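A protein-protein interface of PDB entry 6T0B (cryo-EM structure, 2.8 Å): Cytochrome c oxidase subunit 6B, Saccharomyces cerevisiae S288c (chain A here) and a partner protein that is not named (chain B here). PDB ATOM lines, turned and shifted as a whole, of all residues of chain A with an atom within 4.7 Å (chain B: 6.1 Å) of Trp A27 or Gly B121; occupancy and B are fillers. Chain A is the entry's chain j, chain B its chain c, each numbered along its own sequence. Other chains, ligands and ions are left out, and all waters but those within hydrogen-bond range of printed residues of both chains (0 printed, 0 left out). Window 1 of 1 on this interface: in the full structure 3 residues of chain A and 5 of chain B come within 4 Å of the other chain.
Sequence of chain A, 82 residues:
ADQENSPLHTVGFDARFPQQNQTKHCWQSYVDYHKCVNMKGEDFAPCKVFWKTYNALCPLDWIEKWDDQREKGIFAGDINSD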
ATOM      1  N   THR A  23     -25.239 -20.167  21.965  1.00  0.00           N
ATOM      2  CA  THR A  23     -24.971 -18.732  21.912  1.00  0.00           C
ATOM      3  C   THR A  23     -23.916 -18.342  22.934  1.00  0.00           C
ATOM      4  O   THR A  23     -22.956 -17.622  22.621  1.00  0.00           O
ATOM      5  CB  THR A  23     -26.254 -17.948  22.159  1.00  0.00           C
ATOM      6  OG1 THR A  23     -27.248 -18.371  21.230  1.00  0.00           O
ATOM      7  CG2 THR A  23     -26.012 -16.462  21.973  1.00  0.00           C
ATOM      8  N   LYS A  24     -24.058 -18.850  24.154  1.00  0.00           N
ATOM      9  CA  LYS A  24     -23.100 -18.643  25.222  1.00  0.00           C
ATOM     10  C   LYS A  24     -21.899 -19.564  25.117  1.00  0.00           C
ATOM     11  O   LYS A  24     -21.195 -19.750  26.102  1.00  0.00           O
ATOM     12  CB  LYS A  24     -23.779 -18.821  26.579  1.00  0.00           C
ATOM     13  CG  LYS A  24     -24.787 -17.750  26.900  1.00  0.00           C
ATOM     14  CD  LYS A  24     -25.208 -17.791  28.351  1.00  0.00           C
ATOM     15  CE  LYS A  24     -26.447 -16.935  28.572  1.00  0.00           C
ATOM     16  NZ  LYS A  24     -26.896 -16.935  29.991  1.00  0.00           N
ATOM     17  N   HIS A  25     -21.672 -20.185  23.966  1.00  0.00           N
ATOM     18  CA  HIS A  25     -20.381 -20.773  23.653  1.00  0.00           C
ATOM     19  C   HIS A  25     -19.499 -19.746  22.960  1.00  0.00           C
ATOM     20  O   HIS A  25     -18.380 -19.469  23.403  1.00  0.00           O
ATOM     21  CB  HIS A  25     -20.571 -22.008  22.770  1.00  0.00           C
ATOM     22  CG  HIS A  25     -19.492 -23.035  22.916  1.00  0.00           C
ATOM     23  ND1 HIS A  25     -19.484 -24.209  22.194  1.00  0.00           N
ATOM     24  CD2 HIS A  25     -18.386 -23.065  23.694  1.00  0.00           C
ATOM     25  CE1 HIS A  25     -18.420 -24.918  22.523  1.00  0.00           C
ATOM     26  NE2 HIS A  25     -17.737 -24.248  23.432  1.00  0.00           N
ATOM     27  N   CYS A  26     -20.025 -19.125  21.906  1.00  0.00           N
ATOM     28  CA  CYS A  26     -19.248 -18.128  21.185  1.00  0.00           C
ATOM     29  C   CYS A  26     -19.131 -16.841  21.984  1.00  0.00           C
ATOM     30  O   CYS A  26     -18.064 -16.216  21.981  1.00  0.00           O
ATOM     31  CB  CYS A  26     -19.862 -17.852  19.813  1.00  0.00           C
ATOM     32  SG  CYS A  26     -21.048 -16.504  19.733  1.00  0.00           S
ATOM     33  N   TRP A  27     -20.193 -16.442  22.702  1.00  0.00           N
ATOM     34  CA  TRP A  27     -20.095 -15.235  23.521  1.00  0.00           C
ATOM     35  C   TRP A  27     -19.159 -15.431  24.701  1.00  0.00           C
ATOM     36  O   TRP A  27     -18.389 -14.524  25.041  1.00  0.00           O
ATOM     37  CB  TRP A  27     -21.465 -14.802  24.025  1.00  0.00           C
ATOM     38  CG  TRP A  27     -21.398 -13.596  24.931  1.00  0.00           C
ATOM     39  CD1 TRP A  27     -21.311 -12.294  24.547  1.00  0.00           C
ATOM     40  CD2 TRP A  27     -21.421 -13.588  26.363  1.00  0.00           C
ATOM     41  NE1 TRP A  27     -21.275 -11.479  25.645  1.00  0.00           N
ATOM     42  CE2 TRP A  27     -21.338 -12.249  26.773  1.00  0.00           C
ATOM     43  CE3 TRP A  27     -21.497 -14.586  27.337  1.00  0.00           C
ATOM     44  CZ2 TRP A  27     -21.334 -11.879  28.110  1.00  0.00           C
ATOM     45  CZ3 TRP A  27     -21.492 -14.216  28.663  1.00  0.00           C
ATOM     46  CH2 TRP A  27     -21.408 -12.875  29.038  1.00  0.00           C
ATOM     47  N   GLN A  28     -19.210 -16.602  25.334  1.00  0.00           N
ATOM     48  CA  GLN A  28     -18.326 -16.845  26.460  1.00  0.00           C
ATOM     49  C   GLN A  28     -16.891 -16.973  26.007  1.00  0.00           C
ATOM     50  O   GLN A  28     -16.001 -16.443  26.664  1.00  0.00           O
ATOM     51  CB  GLN A  28     -18.733 -18.092  27.224  1.00  0.00           C
ATOM     52  CG  GLN A  28     -19.534 -17.816  28.475  1.00  0.00           C
ATOM     53  CD  GLN A  28     -18.745 -17.074  29.527  1.00  0.00           C
ATOM     54  OE1 GLN A  28     -17.533 -17.250  29.660  1.00  0.00           O
ATOM     55  NE2 GLN A  28     -19.432 -16.241  30.290  1.00  0.00           N
ATOM     56  N   SER A  29     -16.637 -17.631  24.870  1.00  0.00           N
ATOM     57  CA  SER A  29     -15.261 -17.728  24.405  1.00  0.00           C
ATOM     58  C   SER A  29     -14.729 -16.396  23.886  1.00  0.00           C
ATOM     59  O   SER A  29     -13.530 -16.128  24.027  1.00  0.00           O
ATOM     60  CB  SER A  29     -15.159 -18.796  23.326  1.00  0.00           C
ATOM     61  OG  SER A  29     -15.569 -20.040  23.854  1.00  0.00           O
ATOM     62  N   TYR A  30     -15.604 -15.533  23.361  1.00  0.00           N
ATOM     63  CA  TYR A  30     -15.204 -14.183  22.979  1.00  0.00           C
ATOM     64  C   TYR A  30     -14.834 -13.355  24.200  1.00  0.00           C
ATOM     65  O   TYR A  30     -13.801 -12.672  24.208  1.00  0.00           O
ATOM     66  CB  TYR A  30     -16.340 -13.511  22.202  1.00  0.00           C
ATOM     67  CG  TYR A  30     -16.048 -12.095  21.756  1.00  0.00           C
ATOM     68  CD1 TYR A  30     -15.365 -11.853  20.577  1.00  0.00           C
ATOM     69  CD2 TYR A  30     -16.468 -11.002  22.506  1.00  0.00           C
ATOM     70  CE1 TYR A  30     -15.093 -10.569  20.166  1.00  0.00           C
ATOM     71  CE2 TYR A  30     -16.190  -9.719  22.105  1.00  0.00           C
ATOM     72  CZ  TYR A  30     -15.504  -9.512  20.936  1.00  0.00           C
ATOM     73  OH  TYR A  30     -15.238  -8.234  20.536  1.00  0.00           O
ATOM     74  N   VAL A  31     -15.689 -13.370  25.231  1.00  0.00           N
ATOM     75  CA  VAL A  31     -15.399 -12.557  26.411  1.00  0.00           C
ATOM     76  C   VAL A  31     -14.224 -13.156  27.176  1.00  0.00           C
ATOM     77  O   VAL A  31     -13.429 -12.424  27.777  1.00  0.00           O
ATOM     78  CB  VAL A  31     -16.656 -12.365  27.293  1.00  0.00           C
ATOM     79  CG1 VAL A  31     -17.056 -13.634  28.018  1.00  0.00           C
ATOM     80  CG2 VAL A  31     -16.446 -11.227  28.283  1.00  0.00           C
ATOM     81  N   TRP A  66     -19.406  -6.874  18.167  1.00  0.00           N
ATOM     82  CA  TRP A  66     -18.849  -6.879  19.510  1.00  0.00           C
ATOM     83  C   TRP A  66     -17.496  -6.185  19.570  1.00  0.00           C
ATOM     84  O   TRP A  66     -17.169  -5.565  20.587  1.00  0.00           O
ATOM     85  CB  TRP A  66     -18.729  -8.306  20.021  1.00  0.00           C
ATOM     86  CG  TRP A  66     -20.030  -8.972  20.269  1.00  0.00           C
ATOM     87  CD1 TRP A  66     -21.250  -8.381  20.347  1.00  0.00           C
ATOM     88  CD2 TRP A  66     -20.243 -10.369  20.467  1.00  0.00           C
ATOM     89  NE1 TRP A  66     -22.217  -9.325  20.582  1.00  0.00           N
ATOM     90  CE2 TRP A  66     -21.620 -10.556  20.660  1.00  0.00           C
ATOM     91  CE3 TRP A  66     -19.402 -11.482  20.501  1.00  0.00           C
ATOM     92  CZ2 TRP A  66     -22.177 -11.809  20.881  1.00  0.00           C
ATOM     93  CZ3 TRP A  66     -19.953 -12.720  20.723  1.00  0.00           C
ATOM     94  CH2 TRP A  66     -21.327 -12.875  20.909  1.00  0.00           C
ATOM     95  N   PHE A  75     -19.573  -2.522  25.126  1.00  0.00           N
ATOM     96  CA  PHE A  75     -19.563  -3.968  25.296  1.00  0.00           C
ATOM     97  C   PHE A  75     -20.033  -4.359  26.690  1.00  0.00           C
ATOM     98  O   PHE A  75     -19.553  -3.831  27.696  1.00  0.00           O
ATOM     99  CB  PHE A  75     -18.182  -4.557  25.043  1.00  0.00           C
ATOM    100  CG  PHE A  75     -18.192  -6.058  24.971  1.00  0.00           C
ATOM    101  CD1 PHE A  75     -19.177  -6.708  24.248  1.00  0.00           C
ATOM    102  CD2 PHE A  75     -17.255  -6.816  25.642  1.00  0.00           C
ATOM    103  CE1 PHE A  75     -19.217  -8.076  24.182  1.00  0.00           C
ATOM    104  CE2 PHE A  75     -17.292  -8.190  25.574  1.00  0.00           C
ATOM    105  CZ  PHE A  75     -18.276  -8.815  24.841  1.00  0.00           C
ATOM    106  N   ALA A  76     -20.977  -5.293  26.737  1.00  0.00           N
ATOM    107  CA  ALA A  76     -21.632  -5.714  27.964  1.00  0.00           C
ATOM    108  C   ALA A  76     -20.902  -6.844  28.690  1.00  0.00           C
ATOM    109  O   ALA A  76     -21.505  -7.504  29.537  1.00  0.00           O
ATOM    110  CB  ALA A  76     -23.071  -6.126  27.656  1.00  0.00           C
ATOM    111  N   PRO B 116     -30.574 -14.605  31.039  1.00  0.00           N
ATOM    112  CA  PRO B 116     -30.688 -13.444  30.163  1.00  0.00           C
ATOM    113  C   PRO B 116     -29.857 -13.607  28.905  1.00  0.00           C
ATOM    114  O   PRO B 116     -29.216 -14.631  28.663  1.00  0.00           O
ATOM    115  CB  PRO B 116     -30.169 -12.299  31.026  1.00  0.00           C
ATOM    116  CG  PRO B 116     -29.237 -12.943  31.946  1.00  0.00           C
ATOM    117  CD  PRO B 116     -29.784 -14.298  32.244  1.00  0.00           C
ATOM    118  N   ASP B 117     -29.860 -12.550  28.102  1.00  0.00           N
ATOM    119  CA  ASP B 117     -29.184 -12.582  26.817  1.00  0.00           C
ATOM    120  C   ASP B 117     -27.683 -12.453  26.944  1.00  0.00           C
ATOM    121  O   ASP B 117     -27.115 -12.528  28.037  1.00  0.00           O
ATOM    122  CB  ASP B 117     -29.656 -11.452  25.910  1.00  0.00           C
ATOM    123  CG  ASP B 117     -31.131 -11.474  25.677  1.00  0.00           C
ATOM    124  OD1 ASP B 117     -31.817 -12.353  26.236  1.00  0.00           O
ATOM    125  OD2 ASP B 117     -31.605 -10.622  24.909  1.00  0.00           O
ATOM    126  N   VAL B 118     -27.041 -12.270  25.795  1.00  0.00           N
ATOM    127  CA  VAL B 118     -25.671 -11.802  25.743  1.00  0.00           C
ATOM    128  C   VAL B 118     -25.602 -10.331  25.384  1.00  0.00           C
ATOM    129  O   VAL B 118     -24.554  -9.703  25.593  1.00  0.00           O
ATOM    130  CB  VAL B 118     -24.854 -12.654  24.753  1.00  0.00           C
ATOM    131  CG1 VAL B 118     -24.878 -14.099  25.200  1.00  0.00           C
ATOM    132  CG2 VAL B 118     -25.423 -12.528  23.357  1.00  0.00           C
ATOM    133  N   THR B 119     -26.691  -9.751  24.878  1.00  0.00           N
ATOM    134  CA  THR B 119     -26.703  -8.342  24.512  1.00  0.00           C
ATOM    135  C   THR B 119     -26.957  -7.430  25.699  1.00  0.00           C
ATOM    136  O   THR B 119     -26.746  -6.218  25.589  1.00  0.00           O
ATOM    137  CB  THR B 119     -27.751  -8.074  23.429  1.00  0.00           C
ATOM    138  OG1 THR B 119     -27.644  -6.715  22.997  1.00  0.00           O
ATOM    139  CG2 THR B 119     -29.146  -8.324  23.941  1.00  0.00           C
ATOM    140  N   LEU B 120     -27.404  -7.984  26.820  1.00  0.00           N
ATOM    141  CA  LEU B 120     -27.414  -7.265  28.081  1.00  0.00           C
ATOM    142  C   LEU B 120     -26.200  -7.611  28.923  1.00  0.00           C
ATOM    143  O   LEU B 120     -25.776  -6.802  29.754  1.00  0.00           O
ATOM    144  CB  LEU B 120     -28.694  -7.575  28.859  1.00  0.00           C
ATOM    145  CG  LEU B 120     -30.001  -7.668  28.074  1.00  0.00           C
ATOM    146  CD1 LEU B 120     -31.112  -8.072  29.003  1.00  0.00           C
ATOM    147  CD2 LEU B 120     -30.338  -6.354  27.409  1.00  0.00           C
ATOM    148  N   GLY B 121     -25.636  -8.799  28.727  1.00  0.00           N
ATOM    149  CA  GLY B 121     -24.365  -9.138  29.326  1.00  0.00           C
ATOM    150  C   GLY B 121     -24.375 -10.304  30.285  1.00  0.00           C
ATOM    151  O   GLY B 121     -23.509 -10.370  31.165  1.00  0.00           O
ATOM    152  N   ALA B 122     -25.312 -11.238  30.086  1.00  0.00           N
ATOM    153  CA  ALA B 122     -25.612 -12.329  31.020  1.00  0.00           C
ATOM    154  C   ALA B 122     -25.833 -11.782  32.426  1.00  0.00           C
ATOM    155  O   ALA B 122     -25.261 -12.255  33.410  1.00  0.00           O
ATOM    156  CB  ALA B 122     -24.526 -13.407  31.003  1.00  0.00           C
ATOM    157  N   CYS B 123     -26.675 -10.758  32.504  1.00  0.00           N
ATOM    158  CA  CYS B 123     -26.802  -9.935  33.691  1.00  0.00           C
ATOM    159  C   CYS B 123     -28.266  -9.596  33.897  1.00  0.00           C
ATOM    160  O   CYS B 123     -29.029  -9.486  32.935  1.00  0.00           O
ATOM    161  CB  CYS B 123     -25.968  -8.661  33.542  1.00  0.00           C
ATOM    162  SG  CYS B 123     -25.896  -7.613  34.986  1.00  0.00           S
ATOM    163  N   VAL B 127     -26.687  -4.009  32.377  1.00  0.00           N
ATOM    164  CA  VAL B 127     -25.628  -3.061  32.669  1.00  0.00           C
ATOM    165  C   VAL B 127     -26.075  -1.662  32.280  1.00  0.00           C
ATOM    166  O   VAL B 127     -26.805  -1.467  31.301  1.00  0.00           O
ATOM    167  CB  VAL B 127     -24.332  -3.482  31.955  1.00  0.00           C
ATOM    168  CG1 VAL B 127     -23.853  -4.810  32.503  1.00  0.00           C
ATOM    169  CG2 VAL B 127     -24.543  -3.610  30.456  1.00  0.00           C
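The backbone carbonyl oxygen (O) of Asp B117 is in hydrogen-bond range of the backbone NH (N) of Ala B122 (3.0 Å).
Among the printed residues, pairs that only touch across the chains: Ala A76 with Gly B121 (3.3 Å), Ala A76 with Leu B120 (3.5 Å), Trp A27 with Val B118 (3.5 Å), Lys A24 with Pro B116 (3.5 Å), Trp A27 with Ala B122 (3.7 Å) and Trp A27 with Gly B121 (3.9 Å).
Printed residues of chain B within 4 Å of Lys A24: Pro B116.
Trp A27 touches just these residues of chain B: Val B118, Gly B121 and Ala B122.
Of chain A, only Trp A27 and Ala A76 come within 4 Å of Gly B121.
Of the printed residues of chain A, Ala B122 touches Trp A27.
Val B127 touches none of the printed residues of chain A.
The nearest residue of chain B that does not touch Trp A27 is Thr B119 (5.7 Å).
The nearest printed residue of chain A that does not touch Gly B121 is Phe A75 (7.0 Å).
The nearest printed residue of chain A that does not touch Pro B116 is Thr A23 (7.6 Å).
Printed residues of chain B that touch a printed residue of chain A: Pro B116, Val B118, Leu B120, Gly B121 and Ala B122.
Hydrophobic or aromatic side chains of chain B that line the printed part of chain A: Val B118 and Ala B122.
Of the 12 printed residues of chain A, 3 touch a printed residue of chain B.
Hydrophobic or aromatic side chains of chain A within 4 Å of the printed part of chain B: Trp A27 and Ala A76.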
